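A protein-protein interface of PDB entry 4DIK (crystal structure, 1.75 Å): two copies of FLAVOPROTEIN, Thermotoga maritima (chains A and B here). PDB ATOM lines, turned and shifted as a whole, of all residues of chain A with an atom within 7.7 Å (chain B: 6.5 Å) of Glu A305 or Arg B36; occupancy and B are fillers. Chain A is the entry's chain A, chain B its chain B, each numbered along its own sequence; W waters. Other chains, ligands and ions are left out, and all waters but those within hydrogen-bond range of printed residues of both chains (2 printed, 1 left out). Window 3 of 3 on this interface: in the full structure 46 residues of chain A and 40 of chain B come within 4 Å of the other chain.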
ATOM      1  N   SER A 274      -5.443   3.038   8.115  1.00  0.00           N
ATOM      2  CA  SER A 274      -5.768   1.654   8.397  1.00  0.00           C
ATOM      3  C   SER A 274      -4.733   0.847   7.652  1.00  0.00           C
ATOM      4  O   SER A 274      -4.863   0.636   6.441  1.00  0.00           O
ATOM      5  CB  SER A 274      -7.177   1.315   7.916  1.00  0.00           C
ATOM      6  OG  SER A 274      -7.536   0.007   8.329  1.00  0.00           O
ATOM      7  N   LYS A 301      -9.507   8.479   4.505  1.00  0.00           N
ATOM      8  CA  LYS A 301      -8.883   7.248   4.959  1.00  0.00           C
ATOM      9  C   LYS A 301      -7.643   6.914   4.134  1.00  0.00           C
ATOM     10  O   LYS A 301      -7.659   6.963   2.903  1.00  0.00           O
ATOM     11  CB  LYS A 301      -9.901   6.101   5.000  1.00  0.00           C
ATOM     12  CG  LYS A 301     -10.348   5.564   3.655  1.00  0.00           C
ATOM     13  CD  LYS A 301     -10.760   4.065   3.788  1.00  0.00           C
ATOM     14  CE  LYS A 301      -9.723   3.307   4.648  1.00  0.00           C
ATOM     15  NZ  LYS A 301      -9.844   1.793   4.820  1.00  0.00           N
ATOM     16  N   PHE A 302      -6.541   6.667   4.828  1.00  0.00           N
ATOM     17  CA  PHE A 302      -5.315   6.229   4.178  1.00  0.00           C
ATOM     18  C   PHE A 302      -5.320   4.729   4.299  1.00  0.00           C
ATOM     19  O   PHE A 302      -5.203   4.208   5.405  1.00  0.00           O
ATOM     20  CB  PHE A 302      -4.102   6.767   4.921  1.00  0.00           C
ATOM     21  CG  PHE A 302      -3.925   8.246   4.788  1.00  0.00           C
ATOM     22  CD1 PHE A 302      -3.311   8.770   3.671  1.00  0.00           C
ATOM     23  CD2 PHE A 302      -4.378   9.102   5.785  1.00  0.00           C
ATOM     24  CE1 PHE A 302      -3.129  10.133   3.535  1.00  0.00           C
ATOM     25  CE2 PHE A 302      -4.198  10.490   5.664  1.00  0.00           C
ATOM     26  CZ  PHE A 302      -3.588  10.994   4.533  1.00  0.00           C
ATOM     27  N   SER A 303      -5.464   4.018   3.186  1.00  0.00           N
ATOM     28  CA  SER A 303      -5.458   2.559   3.254  1.00  0.00           C
ATOM     29  C   SER A 303      -4.438   2.000   2.285  1.00  0.00           C
ATOM     30  O   SER A 303      -3.680   2.741   1.665  1.00  0.00           O
ATOM     31  CB  SER A 303      -6.825   1.995   2.880  1.00  0.00           C
ATOM     32  OG  SER A 303      -7.069   2.224   1.512  1.00  0.00           O
ATOM     33  N   ASP A 304      -4.439   0.684   2.116  1.00  0.00           N
ATOM     34  CA  ASP A 304      -3.491   0.098   1.181  1.00  0.00           C
ATOM     35  C   ASP A 304      -3.942   0.283  -0.276  1.00  0.00           C
ATOM     36  O   ASP A 304      -3.215  -0.076  -1.208  1.00  0.00           O
ATOM     37  CB  ASP A 304      -3.170  -1.371   1.548  1.00  0.00           C
ATOM     38  CG  ASP A 304      -4.389  -2.277   1.528  1.00  0.00           C
ATOM     39  OD1 ASP A 304      -5.382  -1.935   0.855  1.00  0.00           O
ATOM     40  OD2 ASP A 304      -4.342  -3.367   2.162  1.00  0.00           O
ATOM     41  N   GLU A 305      -5.123   0.876  -0.460  1.00  0.00           N
ATOM     42  CA  GLU A 305      -5.694   1.126  -1.787  1.00  0.00           C
ATOM     43  C   GLU A 305      -5.995   2.605  -2.083  1.00  0.00           C
ATOM     44  O   GLU A 305      -6.050   3.030  -3.246  1.00  0.00           O
ATOM     45  CB  GLU A 305      -6.973   0.273  -1.971  1.00  0.00           C
ATOM     46  CG  GLU A 305      -6.651  -1.125  -2.340  1.00  0.00           C
ATOM     47  CD  GLU A 305      -7.847  -1.943  -2.815  1.00  0.00           C
ATOM     48  OE1 GLU A 305      -8.913  -1.365  -3.143  1.00  0.00           O
ATOM     49  OE2 GLU A 305      -7.694  -3.160  -2.886  1.00  0.00           O
ATOM     50  N   GLU A 306      -6.198   3.391  -1.031  1.00  0.00           N
ATOM     51  CA  GLU A 306      -6.615   4.780  -1.193  1.00  0.00           C
ATOM     52  C   GLU A 306      -5.760   5.747  -0.388  1.00  0.00           C
ATOM     53  O   GLU A 306      -5.224   5.411   0.668  1.00  0.00           O
ATOM     54  CB  GLU A 306      -8.092   4.934  -0.810  1.00  0.00           C
ATOM     55  CG  GLU A 306      -9.033   3.967  -1.546  1.00  0.00           C
ATOM     56  CD  GLU A 306     -10.486   4.344  -1.367  1.00  0.00           C
ATOM     57  OE1 GLU A 306     -10.949   4.387  -0.197  1.00  0.00           O
ATOM     58  OE2 GLU A 306     -11.160   4.645  -2.394  1.00  0.00           O
ATOM     59  N   ARG A 307      -5.655   6.961  -0.904  1.00  0.00           N
ATOM     60  CA  ARG A 307      -4.784   7.965  -0.327  1.00  0.00           C
ATOM     61  C   ARG A 307      -5.376   9.352  -0.602  1.00  0.00           C
ATOM     62  O   ARG A 307      -5.287   9.854  -1.732  1.00  0.00           O
ATOM     63  CB  ARG A 307      -3.420   7.800  -0.998  1.00  0.00           C
ATOM     64  CG  ARG A 307      -2.479   8.963  -0.986  1.00  0.00           C
ATOM     65  CD  ARG A 307      -1.580   8.915   0.200  1.00  0.00           C
ATOM     66  NE  ARG A 307      -1.116   7.567   0.502  1.00  0.00           N
ATOM     67  CZ  ARG A 307       0.102   7.102   0.232  1.00  0.00           C
ATOM     68  NH1 ARG A 307       1.016   7.880  -0.358  1.00  0.00           N
ATOM     69  NH2 ARG A 307       0.409   5.874   0.608  1.00  0.00           N
ATOM     70  N   HIS B  11     -14.580 -11.557 -15.118  1.00  0.00           N
ATOM     71  CA  HIS B  11     -13.842 -10.428 -14.570  1.00  0.00           C
ATOM     72  C   HIS B  11     -12.429 -10.852 -14.157  1.00  0.00           C
ATOM     73  O   HIS B  11     -12.204 -12.022 -13.849  1.00  0.00           O
ATOM     74  CB  HIS B  11     -14.601  -9.849 -13.371  1.00  0.00           C
ATOM     75  CG  HIS B  11     -14.756 -10.807 -12.231  1.00  0.00           C
ATOM     76  ND1 HIS B  11     -15.551 -11.934 -12.305  1.00  0.00           N
ATOM     77  CD2 HIS B  11     -14.199 -10.819 -10.997  1.00  0.00           C
ATOM     78  CE1 HIS B  11     -15.485 -12.592 -11.156  1.00  0.00           C
ATOM     79  NE2 HIS B  11     -14.670 -11.937 -10.349  1.00  0.00           N
ATOM     80  N   HIS B  12     -11.484  -9.910 -14.169  1.00  0.00           N
ATOM     81  CA  HIS B  12     -10.103 -10.185 -13.770  1.00  0.00           C
ATOM     82  C   HIS B  12     -10.007 -10.669 -12.329  1.00  0.00           C
ATOM     83  O   HIS B  12     -10.653 -10.130 -11.428  1.00  0.00           O
ATOM     84  CB  HIS B  12      -9.213  -8.949 -13.928  1.00  0.00           C
ATOM     85  CG  HIS B  12      -7.829  -9.128 -13.367  1.00  0.00           C
ATOM     86  ND1 HIS B  12      -6.956 -10.092 -13.826  1.00  0.00           N
ATOM     87  CD2 HIS B  12      -7.178  -8.478 -12.368  1.00  0.00           C
ATOM     88  CE1 HIS B  12      -5.820 -10.019 -13.150  1.00  0.00           C
ATOM     89  NE2 HIS B  12      -5.934  -9.057 -12.250  1.00  0.00           N
ATOM     90  N   MET B  13      -9.179 -11.686 -12.123  1.00  0.00           N
ATOM     91  CA  MET B  13      -8.901 -12.188 -10.786  1.00  0.00           C
ATOM     92  C   MET B  13      -7.399 -12.208 -10.555  1.00  0.00           C
ATOM     93  O   MET B  13      -6.625 -12.467 -11.494  1.00  0.00           O
ATOM     94  CB  MET B  13      -9.507 -13.574 -10.625  1.00  0.00           C
ATOM     95  CG  MET B  13     -11.009 -13.568 -10.899  1.00  0.00           C
ATOM     96  SD  MET B  13     -11.816 -15.085 -10.405  1.00  0.00           S
ATOM     97  CE  MET B  13     -10.997 -16.277 -11.419  1.00  0.00           C
ATOM     98  N   PRO B  14      -6.969 -11.917  -9.316  1.00  0.00           N
ATOM     99  CA  PRO B  14      -5.526 -11.995  -9.072  1.00  0.00           C
ATOM    100  C   PRO B  14      -5.004 -13.397  -9.348  1.00  0.00           C
ATOM    101  O   PRO B  14      -5.692 -14.395  -9.067  1.00  0.00           O
ATOM    102  CB  PRO B  14      -5.404 -11.649  -7.587  1.00  0.00           C
ATOM    103  CG  PRO B  14      -6.592 -10.724  -7.338  1.00  0.00           C
ATOM    104  CD  PRO B  14      -7.699 -11.365  -8.160  1.00  0.00           C
ATOM    105  N   ASP B  33      -0.766 -13.289  -6.368  1.00  0.00           N
ATOM    106  CA  ASP B  33      -0.143 -12.056  -6.858  1.00  0.00           C
ATOM    107  C   ASP B  33      -1.095 -10.906  -6.634  1.00  0.00           C
ATOM    108  O   ASP B  33      -2.079 -10.758  -7.355  1.00  0.00           O
ATOM    109  CB  ASP B  33       0.236 -12.209  -8.330  1.00  0.00           C
ATOM    110  CG  ASP B  33       1.386 -13.175  -8.530  1.00  0.00           C
ATOM    111  OD1 ASP B  33       1.933 -13.636  -7.503  1.00  0.00           O
ATOM    112  OD2 ASP B  33       1.735 -13.494  -9.702  1.00  0.00           O
ATOM    113  N   ASP B  34      -0.826 -10.112  -5.600  1.00  0.00           N
ATOM    114  CA  ASP B  34      -1.727  -9.020  -5.260  1.00  0.00           C
ATOM    115  C   ASP B  34      -1.511  -7.839  -6.206  1.00  0.00           C
ATOM    116  O   ASP B  34      -0.556  -7.055  -6.051  1.00  0.00           O
ATOM    117  CB  ASP B  34      -1.551  -8.593  -3.798  1.00  0.00           C
ATOM    118  CG  ASP B  34      -2.608  -7.591  -3.346  1.00  0.00           C
ATOM    119  OD1 ASP B  34      -3.379  -7.116  -4.197  1.00  0.00           O
ATOM    120  OD2 ASP B  34      -2.655  -7.288  -2.134  1.00  0.00           O
ATOM    121  N   ASP B  35      -2.404  -7.712  -7.188  1.00  0.00           N
ATOM    122  CA  ASP B  35      -2.356  -6.580  -8.105  1.00  0.00           C
ATOM    123  C   ASP B  35      -3.432  -5.513  -7.816  1.00  0.00           C
ATOM    124  O   ASP B  35      -3.621  -4.575  -8.601  1.00  0.00           O
ATOM    125  CB  ASP B  35      -2.340  -7.035  -9.585  1.00  0.00           C
ATOM    126  CG  ASP B  35      -3.542  -7.863  -9.968  1.00  0.00           C
ATOM    127  OD1 ASP B  35      -4.546  -7.918  -9.206  1.00  0.00           O
ATOM    128  OD2 ASP B  35      -3.492  -8.504 -11.054  1.00  0.00           O
ATOM    129  N   ARG B  36      -4.102  -5.633  -6.672  1.00  0.00           N
ATOM    130  CA  ARG B  36      -5.076  -4.635  -6.238  1.00  0.00           C
ATOM    131  C   ARG B  36      -4.430  -3.607  -5.320  1.00  0.00           C
ATOM    132  O   ARG B  36      -4.750  -2.418  -5.388  1.00  0.00           O
ATOM    133  CB  ARG B  36      -6.250  -5.271  -5.477  1.00  0.00           C
ATOM    134  CG  ARG B  36      -7.027  -6.343  -6.224  1.00  0.00           C
ATOM    135  CD  ARG B  36      -8.247  -6.831  -5.425  1.00  0.00           C
ATOM    136  NE  ARG B  36      -8.976  -7.863  -6.168  1.00  0.00           N
ATOM    137  CZ  ARG B  36      -9.707  -8.842  -5.634  1.00  0.00           C
ATOM    138  NH1 ARG B  36      -9.846  -8.954  -4.312  1.00  0.00           N
ATOM    139  NH2 ARG B  36     -10.303  -9.724  -6.430  1.00  0.00           N
ATOM    140  N   ILE B  37      -3.542  -4.071  -4.448  1.00  0.00           N
ATOM    141  CA  ILE B  37      -2.885  -3.192  -3.478  1.00  0.00           C
ATOM    142  C   ILE B  37      -2.103  -2.075  -4.182  1.00  0.00           C
ATOM    143  O   ILE B  37      -1.522  -2.291  -5.260  1.00  0.00           O
ATOM    144  CB  ILE B  37      -1.952  -4.004  -2.544  1.00  0.00           C
ATOM    145  CG1 ILE B  37      -1.436  -3.142  -1.380  1.00  0.00           C
ATOM    146  CG2 ILE B  37      -0.755  -4.589  -3.304  1.00  0.00           C
ATOM    147  CD1 ILE B  37      -0.784  -4.019  -0.286  1.00  0.00           C
ATOM    148  N   ARG B  38      -2.096  -0.875  -3.598  1.00  0.00           N
ATOM    149  CA  ARG B  38      -1.337   0.228  -4.175  1.00  0.00           C
ATOM    150  C   ARG B  38      -0.282   0.756  -3.220  1.00  0.00           C
ATOM    151  O   ARG B  38       0.747   1.256  -3.649  1.00  0.00           O
ATOM    152  CB  ARG B  38      -2.280   1.376  -4.587  1.00  0.00           C
ATOM    153  CG  ARG B  38      -3.438   0.902  -5.450  1.00  0.00           C
ATOM    154  CD  ARG B  38      -4.193   2.100  -5.956  1.00  0.00           C
ATOM    155  NE  ARG B  38      -3.265   2.943  -6.684  1.00  0.00           N
ATOM    156  CZ  ARG B  38      -3.481   4.201  -7.017  1.00  0.00           C
ATOM    157  NH1 ARG B  38      -4.623   4.780  -6.698  1.00  0.00           N
ATOM    158  NH2 ARG B  38      -2.556   4.871  -7.686  1.00  0.00           N
ATOM    159  N   TYR B  39      -0.559   0.656  -1.924  1.00  0.00           N
ATOM    160  CA  TYR B  39       0.330   1.206  -0.905  1.00  0.00           C
ATOM    161  C   TYR B  39       0.608   0.144   0.144  1.00  0.00           C
ATOM    162  O   TYR B  39      -0.268  -0.213   0.922  1.00  0.00           O
ATOM    163  CB  TYR B  39      -0.281   2.464  -0.269  1.00  0.00           C
ATOM    164  CG  TYR B  39      -0.782   3.456  -1.290  1.00  0.00           C
ATOM    165  CD1 TYR B  39       0.105   4.181  -2.085  1.00  0.00           C
ATOM    166  CD2 TYR B  39      -2.142   3.635  -1.490  1.00  0.00           C
ATOM    167  CE1 TYR B  39      -0.364   5.088  -3.031  1.00  0.00           C
ATOM    168  CE2 TYR B  39      -2.616   4.515  -2.428  1.00  0.00           C
ATOM    169  CZ  TYR B  39      -1.729   5.239  -3.192  1.00  0.00           C
ATOM    170  OH  TYR B  39      -2.227   6.109  -4.120  1.00  0.00           O
ATOM    171  N   ALA B  42      -0.075   0.650   3.741  1.00  0.00           N
ATOM    172  CA  ALA B  42      -0.805   1.905   3.537  1.00  0.00           C
ATOM    173  C   ALA B  42       0.090   3.135   3.288  1.00  0.00           C
ATOM    174  O   ALA B  42      -0.364   4.279   3.374  1.00  0.00           O
ATOM    175  CB  ALA B  42      -1.806   2.177   4.694  1.00  0.00           C
ATOM    176  N   LYS B  70      -2.971 -12.644   2.851  1.00  0.00           N
ATOM    177  CA  LYS B  70      -3.667 -11.465   3.367  1.00  0.00           C
ATOM    178  C   LYS B  70      -5.170 -11.742   3.489  1.00  0.00           C
ATOM    179  O   LYS B  70      -5.744 -12.543   2.733  1.00  0.00           O
ATOM    180  CB  LYS B  70      -3.398 -10.289   2.421  1.00  0.00           C
ATOM    181  CG  LYS B  70      -3.826  -8.919   2.919  1.00  0.00           C
ATOM    182  CD  LYS B  70      -3.334  -7.889   1.873  1.00  0.00           C
ATOM    183  CE  LYS B  70      -3.743  -6.488   2.192  1.00  0.00           C
ATOM    184  NZ  LYS B  70      -5.007  -6.166   1.485  1.00  0.00           N
ATOM    185  N   ASN B  72      -8.039 -10.347   2.882  1.00  0.00           N
ATOM    186  CA  ASN B  72      -9.013 -10.136   1.814  1.00  0.00           C
ATOM    187  C   ASN B  72      -8.990 -11.251   0.760  1.00  0.00           C
ATOM    188  O   ASN B  72      -9.840 -11.298  -0.134  1.00  0.00           O
ATOM    189  CB  ASN B  72      -8.851  -8.742   1.163  1.00  0.00           C
ATOM    190  CG  ASN B  72      -7.474  -8.533   0.524  1.00  0.00           C
ATOM    191  OD1 ASN B  72      -6.454  -9.005   1.036  1.00  0.00           O
ATOM    192  ND2 ASN B  72      -7.448  -7.827  -0.608  1.00  0.00           N
ATOM    193  N   TYR B  73      -8.018 -12.154   0.879  1.00  0.00           N
ATOM    194  CA  TYR B  73      -7.893 -13.305  -0.013  1.00  0.00           C
ATOM    195  C   TYR B  73      -8.063 -14.634   0.734  1.00  0.00           C
ATOM    196  O   TYR B  73      -7.627 -15.683   0.265  1.00  0.00           O
ATOM    197  CB  TYR B  73      -6.545 -13.291  -0.749  1.00  0.00           C
ATOM    198  CG  TYR B  73      -6.345 -12.071  -1.623  1.00  0.00           C
ATOM    199  CD1 TYR B  73      -7.232 -11.774  -2.648  1.00  0.00           C
ATOM    200  CD2 TYR B  73      -5.278 -11.208  -1.404  1.00  0.00           C
ATOM    201  CE1 TYR B  73      -7.064 -10.631  -3.443  1.00  0.00           C
ATOM    202  CE2 TYR B  73      -5.095 -10.076  -2.194  1.00  0.00           C
ATOM    203  CZ  TYR B  73      -5.988  -9.794  -3.210  1.00  0.00           C
ATOM    204  OH  TYR B  73      -5.805  -8.657  -3.985  1.00  0.00           O
ATOM    205  N   GLU B  76      -9.917 -17.238  -1.343  1.00  0.00           N
ATOM    206  CA  GLU B  76      -9.077 -17.738  -2.421  1.00  0.00           C
ATOM    207  C   GLU B  76      -8.020 -18.675  -1.853  1.00  0.00           C
ATOM    208  O   GLU B  76      -7.632 -19.648  -2.493  1.00  0.00           O
ATOM    209  CB  GLU B  76      -8.403 -16.576  -3.170  1.00  0.00           C
ATOM    210  CG  GLU B  76      -9.341 -15.716  -4.027  1.00  0.00           C
ATOM    211  CD  GLU B  76      -9.984 -14.585  -3.248  1.00  0.00           C
ATOM    212  OE1 GLU B  76     -10.014 -14.642  -1.997  1.00  0.00           O
ATOM    213  OE2 GLU B  76     -10.468 -13.631  -3.892  1.00  0.00           O
HETATM  214  O   HOH W   1      -5.163   7.046  -4.284  1.00  0.00           O
HETATM  215  O   HOH W   2      -7.310  -4.064   1.300  1.00  0.00           O
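The backbone carbonyl oxygen of Asp A304 sits at hydrogen-bond distance from the backbone NH of Arg B38, 2.8 Å away.
O of Asp A304 is in hydrogen-bond range of N of Tyr B39 (2.8 Å).
The side-chain carboxylate (OD2) of Asp A304 lies within salt-bridge range of the side-chain amino group (NZ) of Lys B70 (3.0 Å).
NH2 of Arg A307 sits at hydrogen-bond distance from O of Ala B42, 3.3 Å away.
The backbone carbonyl oxygen of Phe A302 sits at hydrogen-bond distance from the backbone NH of Ser A274.
The backbone NH of Glu A305 lies close to the side-chain hydroxyl of Ser A303 (3.1 Å).
The backbone NH of Glu A306 lies within hydrogen-bond range of the side-chain hydroxyl of Ser A303 (2.9 Å).
OD1 of Asp B34 is in hydrogen-bond range of N of Arg B36 (3.0 Å).
N of Ile B37 sits at hydrogen-bond distance from OD1 of Asp B34, at 3.1 Å.
The side-chain amino group of Lys B70 is in hydrogen-bond range of the side-chain amide oxygen of Asn B72.
Ala B42 touches Ser A274.
Tyr B39 touches Ser A303 (CD2 to O, 3.6 Å).
Ala B42 touches Ser A303.
Ile B37 touches Asp A304.
Ala B42 touches Asp A304 (CB to N, 3.98 Å).
Glu A305 touches Arg B36 (OE2 to CB, 3.6 Å).
Glu A305 touches Arg B38.
Glu A305 touches Tyr B39.
C of Glu A306 touches CE2 of Tyr B39, at 3.9 Å.
NH2 of Arg A307 touches CD1 of Tyr B39 (3.2 Å).
Of chain B, only Arg B36 (3.6 Å), Arg B38 (3.4 Å) and Tyr B39 (3.8 Å) come within 4 Å of Glu A305.
Of the printed residues of chain A, Ile B37 touches Asp A304 (3.5 Å).
Of the printed residues of chain A, Arg B38 touches Asp A304 and Glu A305.
Of the printed residues of chain A, Lys B70 touches Asp A304.
The nearest residue of chain B that does not touch Glu A305 is Ile B37 (4.4 Å).
The nearest residue of chain A that does not touch Arg B36 is Asp A304 (5.0 Å).
Of the 8 printed residues of chain A, 6 touch a printed residue of chain B.
Printed residues of chain B that touch a printed residue of chain A: Arg B36, Ile B37, Arg B38, Tyr B39, Ala B42 and Lys B70.
Among the printed residues, 14 pairs touch across the chains.
Among the printed residues, Asp or Glu carboxylates within 4 Å of a Lys or Arg side-chain nitrogen of the other chain: Asp A304 with Lys B70.
No position is printed for both chains.
Of the 14 pairs that touch across the chains among the printed residues, none has its exchanged pair printed and touching as well.
Water W2 bridges OD1 of Asp A304 (2.9 Å) and NZ of Lys B70 (3.1 Å).
Water W1 lies within hydrogen-bond range of OH of Tyr B39, NH1 of Arg B38 and N of Arg A307.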
